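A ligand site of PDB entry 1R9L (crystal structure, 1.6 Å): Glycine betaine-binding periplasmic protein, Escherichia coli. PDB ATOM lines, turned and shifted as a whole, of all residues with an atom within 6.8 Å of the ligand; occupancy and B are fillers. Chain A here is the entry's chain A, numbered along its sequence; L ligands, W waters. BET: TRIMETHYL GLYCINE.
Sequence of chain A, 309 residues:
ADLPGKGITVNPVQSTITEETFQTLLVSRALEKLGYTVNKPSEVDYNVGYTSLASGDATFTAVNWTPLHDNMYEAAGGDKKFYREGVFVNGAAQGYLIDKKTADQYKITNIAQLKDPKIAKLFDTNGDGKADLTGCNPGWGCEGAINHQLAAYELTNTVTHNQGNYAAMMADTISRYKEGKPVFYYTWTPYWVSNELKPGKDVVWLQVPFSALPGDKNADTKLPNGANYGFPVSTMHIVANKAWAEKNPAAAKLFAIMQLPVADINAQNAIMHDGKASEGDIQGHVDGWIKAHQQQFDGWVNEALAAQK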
ATOM      1  N   SER A  15     -16.125 -15.193   5.708  1.00  0.00           N
ATOM      2  CA  SER A  15     -17.241 -16.128   5.535  1.00  0.00           C
ATOM      3  C   SER A  15     -18.368 -15.471   4.780  1.00  0.00           C
ATOM      4  O   SER A  15     -18.293 -14.304   4.402  1.00  0.00           O
ATOM      5  CB  SER A  15     -17.716 -16.624   6.892  1.00  0.00           C
ATOM      6  OG  SER A  15     -18.525 -15.668   7.561  1.00  0.00           O
ATOM      7  N   ILE A  17     -20.987 -14.643   6.191  1.00  0.00           N
ATOM      8  CA  ILE A  17     -21.571 -13.723   7.143  1.00  0.00           C
ATOM      9  C   ILE A  17     -21.274 -12.321   6.646  1.00  0.00           C
ATOM     10  O   ILE A  17     -20.139 -11.893   6.717  1.00  0.00           O
ATOM     11  CB  ILE A  17     -20.963 -13.947   8.532  1.00  0.00           C
ATOM     12  CG1 ILE A  17     -21.342 -15.312   9.113  1.00  0.00           C
ATOM     13  CG2 ILE A  17     -21.399 -12.838   9.488  1.00  0.00           C
ATOM     14  CD1 ILE A  17     -20.653 -15.608  10.423  1.00  0.00           C
ATOM     15  N   GLU A  20     -19.396  -9.522   8.450  1.00  0.00           N
ATOM     16  CA  GLU A  20     -17.925  -9.488   8.403  1.00  0.00           C
ATOM     17  C   GLU A  20     -17.355  -8.607   7.286  1.00  0.00           C
ATOM     18  O   GLU A  20     -16.160  -8.327   7.273  1.00  0.00           O
ATOM     19  CB  GLU A  20     -17.351 -10.897   8.232  1.00  0.00           C
ATOM     20  CG  GLU A  20     -17.609 -11.789   9.402  1.00  0.00           C
ATOM     21  CD  GLU A  20     -17.040 -13.181   9.272  1.00  0.00           C
ATOM     22  OE1 GLU A  20     -16.836 -13.645   8.118  1.00  0.00           O
ATOM     23  OE2 GLU A  20     -16.843 -13.833  10.303  1.00  0.00           O
ATOM     24  N   TYR A  46     -15.147 -21.285   6.644  1.00  0.00           N
ATOM     25  CA  TYR A  46     -13.998 -20.831   7.414  1.00  0.00           C
ATOM     26  C   TYR A  46     -12.797 -21.716   7.174  1.00  0.00           C
ATOM     27  O   TYR A  46     -11.705 -21.216   6.954  1.00  0.00           O
ATOM     28  CB  TYR A  46     -14.267 -20.755   8.899  1.00  0.00           C
ATOM     29  CG  TYR A  46     -15.053 -19.551   9.372  1.00  0.00           C
ATOM     30  CD1 TYR A  46     -16.231 -19.718  10.083  1.00  0.00           C
ATOM     31  CD2 TYR A  46     -14.609 -18.249   9.148  1.00  0.00           C
ATOM     32  CE1 TYR A  46     -16.938 -18.645  10.558  1.00  0.00           C
ATOM     33  CE2 TYR A  46     -15.319 -17.177   9.614  1.00  0.00           C
ATOM     34  CZ  TYR A  46     -16.472 -17.392  10.313  1.00  0.00           C
ATOM     35  OH  TYR A  46     -17.191 -16.340  10.815  1.00  0.00           O
ATOM     36  N   VAL A  63     -11.031 -11.928  10.034  1.00  0.00           N
ATOM     37  CA  VAL A  63     -11.992 -12.578  10.938  1.00  0.00           C
ATOM     38  C   VAL A  63     -11.465 -13.845  11.607  1.00  0.00           C
ATOM     39  O   VAL A  63     -12.204 -14.781  11.877  1.00  0.00           O
ATOM     40  CB  VAL A  63     -13.368 -12.847  10.237  1.00  0.00           C
ATOM     41  CG1 VAL A  63     -13.999 -11.511   9.855  1.00  0.00           C
ATOM     42  CG2 VAL A  63     -13.258 -13.796   9.035  1.00  0.00           C
ATOM     43  N   TRP A  65     -10.884 -15.654  14.591  1.00  0.00           N
ATOM     44  CA  TRP A  65     -11.405 -15.590  15.966  1.00  0.00           C
ATOM     45  C   TRP A  65     -10.542 -16.364  16.944  1.00  0.00           C
ATOM     46  O   TRP A  65     -10.126 -17.468  16.668  1.00  0.00           O
ATOM     47  CB  TRP A  65     -12.809 -16.200  16.032  1.00  0.00           C
ATOM     48  CG  TRP A  65     -13.904 -15.280  15.666  1.00  0.00           C
ATOM     49  CD1 TRP A  65     -14.329 -14.939  14.406  1.00  0.00           C
ATOM     50  CD2 TRP A  65     -14.780 -14.624  16.583  1.00  0.00           C
ATOM     51  NE1 TRP A  65     -15.398 -14.074  14.492  1.00  0.00           N
ATOM     52  CE2 TRP A  65     -15.676 -13.852  15.825  1.00  0.00           C
ATOM     53  CE3 TRP A  65     -14.838 -14.549  17.982  1.00  0.00           C
ATOM     54  CZ2 TRP A  65     -16.643 -13.072  16.396  1.00  0.00           C
ATOM     55  CZ3 TRP A  65     -15.811 -13.791  18.547  1.00  0.00           C
ATOM     56  CH2 TRP A  65     -16.700 -13.036  17.758  1.00  0.00           C
ATOM     57  N   LEU A  68     -12.304 -19.276  19.028  1.00  0.00           N
ATOM     58  CA  LEU A  68     -13.124 -20.134  18.207  1.00  0.00           C
ATOM     59  C   LEU A  68     -12.429 -20.773  17.039  1.00  0.00           C
ATOM     60  O   LEU A  68     -12.807 -21.853  16.635  1.00  0.00           O
ATOM     61  CB  LEU A  68     -14.330 -19.380  17.685  1.00  0.00           C
ATOM     62  CG  LEU A  68     -15.367 -18.942  18.709  1.00  0.00           C
ATOM     63  CD1 LEU A  68     -16.389 -18.091  18.034  1.00  0.00           C
ATOM     64  CD2 LEU A  68     -16.040 -20.105  19.345  1.00  0.00           C
ATOM     65  N   HIS A  69     -11.444 -20.095  16.451  1.00  0.00           N
ATOM     66  CA  HIS A  69     -10.730 -20.645  15.287  1.00  0.00           C
ATOM     67  C   HIS A  69      -9.366 -21.236  15.645  1.00  0.00           C
ATOM     68  O   HIS A  69      -8.654 -21.630  14.747  1.00  0.00           O
ATOM     69  CB  HIS A  69     -10.532 -19.560  14.217  1.00  0.00           C
ATOM     70  CG  HIS A  69     -11.799 -19.067  13.588  1.00  0.00           C
ATOM     71  ND1 HIS A  69     -11.823 -18.111  12.613  1.00  0.00           N
ATOM     72  CD2 HIS A  69     -13.083 -19.418  13.806  1.00  0.00           C
ATOM     73  CE1 HIS A  69     -13.070 -17.890  12.233  1.00  0.00           C
ATOM     74  NE2 HIS A  69     -13.854 -18.647  12.969  1.00  0.00           N
ATOM     75  N   MET A  72      -8.818 -24.705  14.093  1.00  0.00           N
ATOM     76  CA  MET A  72      -8.701 -24.638  12.636  1.00  0.00           C
ATOM     77  C   MET A  72      -7.379 -23.997  12.191  1.00  0.00           C
ATOM     78  O   MET A  72      -6.747 -24.429  11.238  1.00  0.00           O
ATOM     79  CB  MET A  72      -9.854 -23.839  12.018  1.00  0.00           C
ATOM     80  CG  MET A  72     -11.114 -24.622  11.882  1.00  0.00           C
ATOM     81  SD  MET A  72     -12.368 -23.650  11.000  1.00  0.00           S
ATOM     82  CE  MET A  72     -12.903 -22.681  12.310  1.00  0.00           C
ATOM     83  N   GLN A  94     -19.103 -13.869  23.724  1.00  0.00           N
ATOM     84  CA  GLN A  94     -19.845 -15.045  23.287  1.00  0.00           C
ATOM     85  C   GLN A  94     -20.552 -15.568  24.497  1.00  0.00           C
ATOM     86  O   GLN A  94     -20.093 -15.383  25.618  1.00  0.00           O
ATOM     87  CB  GLN A  94     -18.895 -16.175  22.891  1.00  0.00           C
ATOM     88  CG  GLN A  94     -17.988 -15.891  21.807  1.00  0.00           C
ATOM     89  CD  GLN A  94     -17.118 -17.035  21.574  1.00  0.00           C
ATOM     90  OE1 GLN A  94     -15.906 -16.958  21.781  1.00  0.00           O
ATOM     91  NE2 GLN A  94     -17.709 -18.127  21.175  1.00  0.00           N
ATOM     92  N   CYS A 136     -25.060 -22.940  16.050  1.00  0.00           N
ATOM     93  CA  CYS A 136     -24.135 -22.490  15.045  1.00  0.00           C
ATOM     94  C   CYS A 136     -24.172 -23.304  13.745  1.00  0.00           C
ATOM     95  O   CYS A 136     -24.350 -24.517  13.739  1.00  0.00           O
ATOM     96  CB  CYS A 136     -22.726 -22.491  15.622  1.00  0.00           C
ATOM     97  SG  CYS A 136     -22.555 -21.188  16.842  1.00  0.00           S
ATOM     98  N   ASN A 137     -23.942 -22.626  12.632  1.00  0.00           N
ATOM     99  CA  ASN A 137     -23.886 -23.304  11.328  1.00  0.00           C
ATOM    100  C   ASN A 137     -22.760 -24.333  11.329  1.00  0.00           C
ATOM    101  O   ASN A 137     -21.703 -24.094  11.911  1.00  0.00           O
ATOM    102  CB  ASN A 137     -23.596 -22.317  10.200  1.00  0.00           C
ATOM    103  CG  ASN A 137     -24.668 -21.241  10.039  1.00  0.00           C
ATOM    104  OD1 ASN A 137     -25.481 -21.022  10.927  1.00  0.00           O
ATOM    105  ND2 ASN A 137     -24.678 -20.592   8.866  1.00  0.00           N
ATOM    106  N   GLY A 139     -19.482 -25.887  10.542  1.00  0.00           N
ATOM    107  CA  GLY A 139     -18.268 -25.264  10.080  1.00  0.00           C
ATOM    108  C   GLY A 139     -17.853 -24.010  10.808  1.00  0.00           C
ATOM    109  O   GLY A 139     -16.717 -23.550  10.643  1.00  0.00           O
ATOM    110  N   TRP A 140     -18.765 -23.422  11.565  1.00  0.00           N
ATOM    111  CA  TRP A 140     -18.406 -22.304  12.412  1.00  0.00           C
ATOM    112  C   TRP A 140     -17.631 -22.839  13.609  1.00  0.00           C
ATOM    113  O   TRP A 140     -17.920 -23.931  14.096  1.00  0.00           O
ATOM    114  CB  TRP A 140     -19.664 -21.596  12.912  1.00  0.00           C
ATOM    115  CG  TRP A 140     -20.321 -20.722  11.869  1.00  0.00           C
ATOM    116  CD1 TRP A 140     -19.964 -20.615  10.544  1.00  0.00           C
ATOM    117  CD2 TRP A 140     -21.486 -19.902  12.032  1.00  0.00           C
ATOM    118  NE1 TRP A 140     -20.800 -19.747   9.894  1.00  0.00           N
ATOM    119  CE2 TRP A 140     -21.739 -19.282  10.790  1.00  0.00           C
ATOM    120  CE3 TRP A 140     -22.309 -19.585  13.111  1.00  0.00           C
ATOM    121  CZ2 TRP A 140     -22.797 -18.399  10.618  1.00  0.00           C
ATOM    122  CZ3 TRP A 140     -23.342 -18.684  12.929  1.00  0.00           C
ATOM    123  CH2 TRP A 140     -23.578 -18.110  11.698  1.00  0.00           C
ATOM    124  N   GLY A 141     -16.648 -22.080  14.108  1.00  0.00           N
ATOM    125  CA  GLY A 141     -15.912 -22.499  15.302  1.00  0.00           C
ATOM    126  C   GLY A 141     -16.818 -22.680  16.500  1.00  0.00           C
ATOM    127  O   GLY A 141     -16.591 -23.572  17.341  1.00  0.00           O
ATOM    128  N   CYS A 142     -17.901 -21.907  16.549  1.00  0.00           N
ATOM    129  CA  CYS A 142     -18.814 -22.030  17.678  1.00  0.00           C
ATOM    130  C   CYS A 142     -19.603 -23.332  17.671  1.00  0.00           C
ATOM    131  O   CYS A 142     -20.099 -23.769  18.711  1.00  0.00           O
ATOM    132  CB  CYS A 142     -19.713 -20.803  17.835  1.00  0.00           C
ATOM    133  SG  CYS A 142     -20.755 -20.355  16.426  1.00  0.00           S
ATOM    134  N   GLU A 143     -19.679 -23.990  16.522  1.00  0.00           N
ATOM    135  CA  GLU A 143     -20.277 -25.320  16.492  1.00  0.00           C
ATOM    136  C   GLU A 143     -19.509 -26.256  17.435  1.00  0.00           C
ATOM    137  O   GLU A 143     -20.083 -26.936  18.275  1.00  0.00           O
ATOM    138  CB  GLU A 143     -20.310 -25.884  15.075  1.00  0.00           C
ATOM    139  CG  GLU A 143     -20.668 -27.359  15.010  1.00  0.00           C
ATOM    140  CD  GLU A 143     -20.540 -27.918  13.606  1.00  0.00           C
ATOM    141  OE1 GLU A 143     -19.492 -27.682  12.937  1.00  0.00           O
ATOM    142  OE2 GLU A 143     -21.476 -28.627  13.203  1.00  0.00           O
ATOM    143  N   TYR A 186     -27.364 -19.179  21.544  1.00  0.00           N
ATOM    144  CA  TYR A 186     -25.980 -18.726  21.609  1.00  0.00           C
ATOM    145  C   TYR A 186     -25.910 -17.521  20.700  1.00  0.00           C
ATOM    146  O   TYR A 186     -26.601 -17.460  19.705  1.00  0.00           O
ATOM    147  CB  TYR A 186     -25.057 -19.826  21.091  1.00  0.00           C
ATOM    148  CG  TYR A 186     -23.684 -19.346  20.693  1.00  0.00           C
ATOM    149  CD1 TYR A 186     -22.651 -19.353  21.587  1.00  0.00           C
ATOM    150  CD2 TYR A 186     -23.433 -18.878  19.419  1.00  0.00           C
ATOM    151  CE1 TYR A 186     -21.378 -18.914  21.234  1.00  0.00           C
ATOM    152  CE2 TYR A 186     -22.184 -18.436  19.063  1.00  0.00           C
ATOM    153  CZ  TYR A 186     -21.181 -18.469  19.970  1.00  0.00           C
ATOM    154  OH  TYR A 186     -19.920 -18.011  19.609  1.00  0.00           O
ATOM    155  N   THR A 187     -25.119 -16.534  21.093  1.00  0.00           N
ATOM    156  CA  THR A 187     -24.738 -15.449  20.220  1.00  0.00           C
ATOM    157  C   THR A 187     -23.361 -14.928  20.542  1.00  0.00           C
ATOM    158  O   THR A 187     -22.750 -15.353  21.534  1.00  0.00           O
ATOM    159  CB  THR A 187     -25.819 -14.337  20.184  1.00  0.00           C
ATOM    160  OG1 THR A 187     -25.696 -13.605  18.970  1.00  0.00           O
ATOM    161  CG2 THR A 187     -25.655 -13.341  21.349  1.00  0.00           C
ATOM    162  N   TRP A 188     -22.893 -14.006  19.704  1.00  0.00           N
ATOM    163  CA  TRP A 188     -21.621 -13.354  19.895  1.00  0.00           C
ATOM    164  C   TRP A 188     -21.795 -11.874  19.618  1.00  0.00           C
ATOM    165  O   TRP A 188     -22.742 -11.455  18.952  1.00  0.00           O
ATOM    166  CB  TRP A 188     -20.571 -13.913  18.955  1.00  0.00           C
ATOM    167  CG  TRP A 188     -20.852 -13.679  17.496  1.00  0.00           C
ATOM    168  CD1 TRP A 188     -20.297 -12.740  16.703  1.00  0.00           C
ATOM    169  CD2 TRP A 188     -21.728 -14.454  16.650  1.00  0.00           C
ATOM    170  NE1 TRP A 188     -20.794 -12.834  15.434  1.00  0.00           N
ATOM    171  CE2 TRP A 188     -21.681 -13.868  15.372  1.00  0.00           C
ATOM    172  CE3 TRP A 188     -22.560 -15.539  16.851  1.00  0.00           C
ATOM    173  CZ2 TRP A 188     -22.403 -14.386  14.299  1.00  0.00           C
ATOM    174  CZ3 TRP A 188     -23.271 -16.046  15.795  1.00  0.00           C
ATOM    175  CH2 TRP A 188     -23.202 -15.455  14.541  1.00  0.00           C
ATOM    176  N   PRO A 190     -19.106  -8.895  17.904  1.00  0.00           N
ATOM    177  CA  PRO A 190     -20.129  -8.052  17.315  1.00  0.00           C
ATOM    178  C   PRO A 190     -21.067  -8.801  16.380  1.00  0.00           C
ATOM    179  O   PRO A 190     -20.611  -9.621  15.603  1.00  0.00           O
ATOM    180  CB  PRO A 190     -19.294  -7.063  16.503  1.00  0.00           C
ATOM    181  CG  PRO A 190     -18.097  -7.789  16.086  1.00  0.00           C
ATOM    182  CD  PRO A 190     -17.832  -8.814  17.175  1.00  0.00           C
ATOM    183  N   TYR A 191     -22.355  -8.489  16.443  1.00  0.00           N
ATOM    184  CA  TYR A 191     -23.360  -9.032  15.524  1.00  0.00           C
ATOM    185  C   TYR A 191     -24.646  -8.254  15.761  1.00  0.00           C
ATOM    186  O   TYR A 191     -24.704  -7.503  16.719  1.00  0.00           O
ATOM    187  CB  TYR A 191     -23.581 -10.528  15.756  1.00  0.00           C
ATOM    188  CG  TYR A 191     -24.300 -11.248  14.655  1.00  0.00           C
ATOM    189  CD1 TYR A 191     -23.780 -11.320  13.365  1.00  0.00           C
ATOM    190  CD2 TYR A 191     -25.502 -11.913  14.907  1.00  0.00           C
ATOM    191  CE1 TYR A 191     -24.445 -11.996  12.358  1.00  0.00           C
ATOM    192  CE2 TYR A 191     -26.149 -12.614  13.898  1.00  0.00           C
ATOM    193  CZ  TYR A 191     -25.624 -12.655  12.635  1.00  0.00           C
ATOM    194  OH  TYR A 191     -26.276 -13.376  11.671  1.00  0.00           O
ATOM    195  N   MET A 236     -10.650 -10.844  17.370  1.00  0.00           N
ATOM    196  CA  MET A 236     -10.364 -11.190  15.986  1.00  0.00           C
ATOM    197  C   MET A 236      -9.041 -10.598  15.547  1.00  0.00           C
ATOM    198  O   MET A 236      -8.654  -9.518  15.937  1.00  0.00           O
ATOM    199  CB  MET A 236     -11.486 -10.726  15.053  1.00  0.00           C
ATOM    200  CG  MET A 236     -12.745 -11.521  15.213  1.00  0.00           C
ATOM    201  SD  MET A 236     -14.163 -10.895  14.287  1.00  0.00           S
ATOM    202  CE  MET A 236     -14.854  -9.745  15.465  1.00  0.00           C
HETATM  203  N   BET L   1     -18.731 -16.631  14.466  1.00  0.00           N
HETATM  204  CA  BET L   1     -17.432 -17.275  14.166  1.00  0.00           C
HETATM  205  C   BET L   1     -17.269 -18.745  14.414  1.00  0.00           C
HETATM  206  O   BET L   1     -16.369 -19.329  13.829  1.00  0.00           O
HETATM  207  OXT BET L   1     -18.073 -19.364  15.213  1.00  0.00           O
HETATM  208  C1  BET L   1     -18.688 -15.292  13.856  1.00  0.00           C
HETATM  209  C2  BET L   1     -19.865 -17.383  13.898  1.00  0.00           C
HETATM  210  C3  BET L   1     -18.846 -16.502  15.940  1.00  0.00           C
HETATM  211  O   HOH W   1     -17.153 -12.635  12.674  1.00  0.00           O
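Water W1 bridges OE2 of Glu 20 (2.7 Å) and NE1 of Trp 65 (2.9 Å).
Merely in contact with the ligand: Trp 140 (3.4 Å), Tyr 46 (3.4 Å), Leu 68 (3.5 Å), Trp 65 (3.6 Å), Trp 188 (3.6 Å) and Ile 17 (3.97 Å).
Nine residues have an atom within 4 Å of the ligand: Ile 17, Tyr 46, Trp 65, Leu 68, His 69, Trp 140, Gly 141, Cys 142 and Trp 188.
The side-chain hydroxyl of Ser 15 sits at hydrogen-bond distance from the backbone NH of Ile 17, 3.0 Å away.
SG of Cys 142 forms a disulfide with SG of Cys 136.
The backbone carbonyl oxygen of Pro 190 sits at hydrogen-bond distance from the indole nitrogen of Trp 188, at 3.2 Å.
The side-chain carboxylate (OE2) of Glu 20 is in hydrogen-bond range of the side-chain hydroxyl (OH) of Tyr 46 (2.6 Å).
A ring nitrogen (ND1) of His 69 sits close to the backbone carbonyl oxygen of Val 63 (3.4 Å).
The side-chain sulfur of Met 236 sits at hydrogen-bond distance from the indole nitrogen of Trp 65 (3.4 Å).
A ring nitrogen (ND1) of His 69 is in hydrogen-bond range of the backbone NH (N) of Trp 65.
The backbone NH (N) of Gly 141 lies within hydrogen-bond range of an oxygen (O) of the ligand (2.8 Å).
N of Cys 142 sits at hydrogen-bond distance from OXT of the ligand (2.9 Å).
NE2 of His 69 is in hydrogen-bond range of O of the ligand (2.7 Å).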
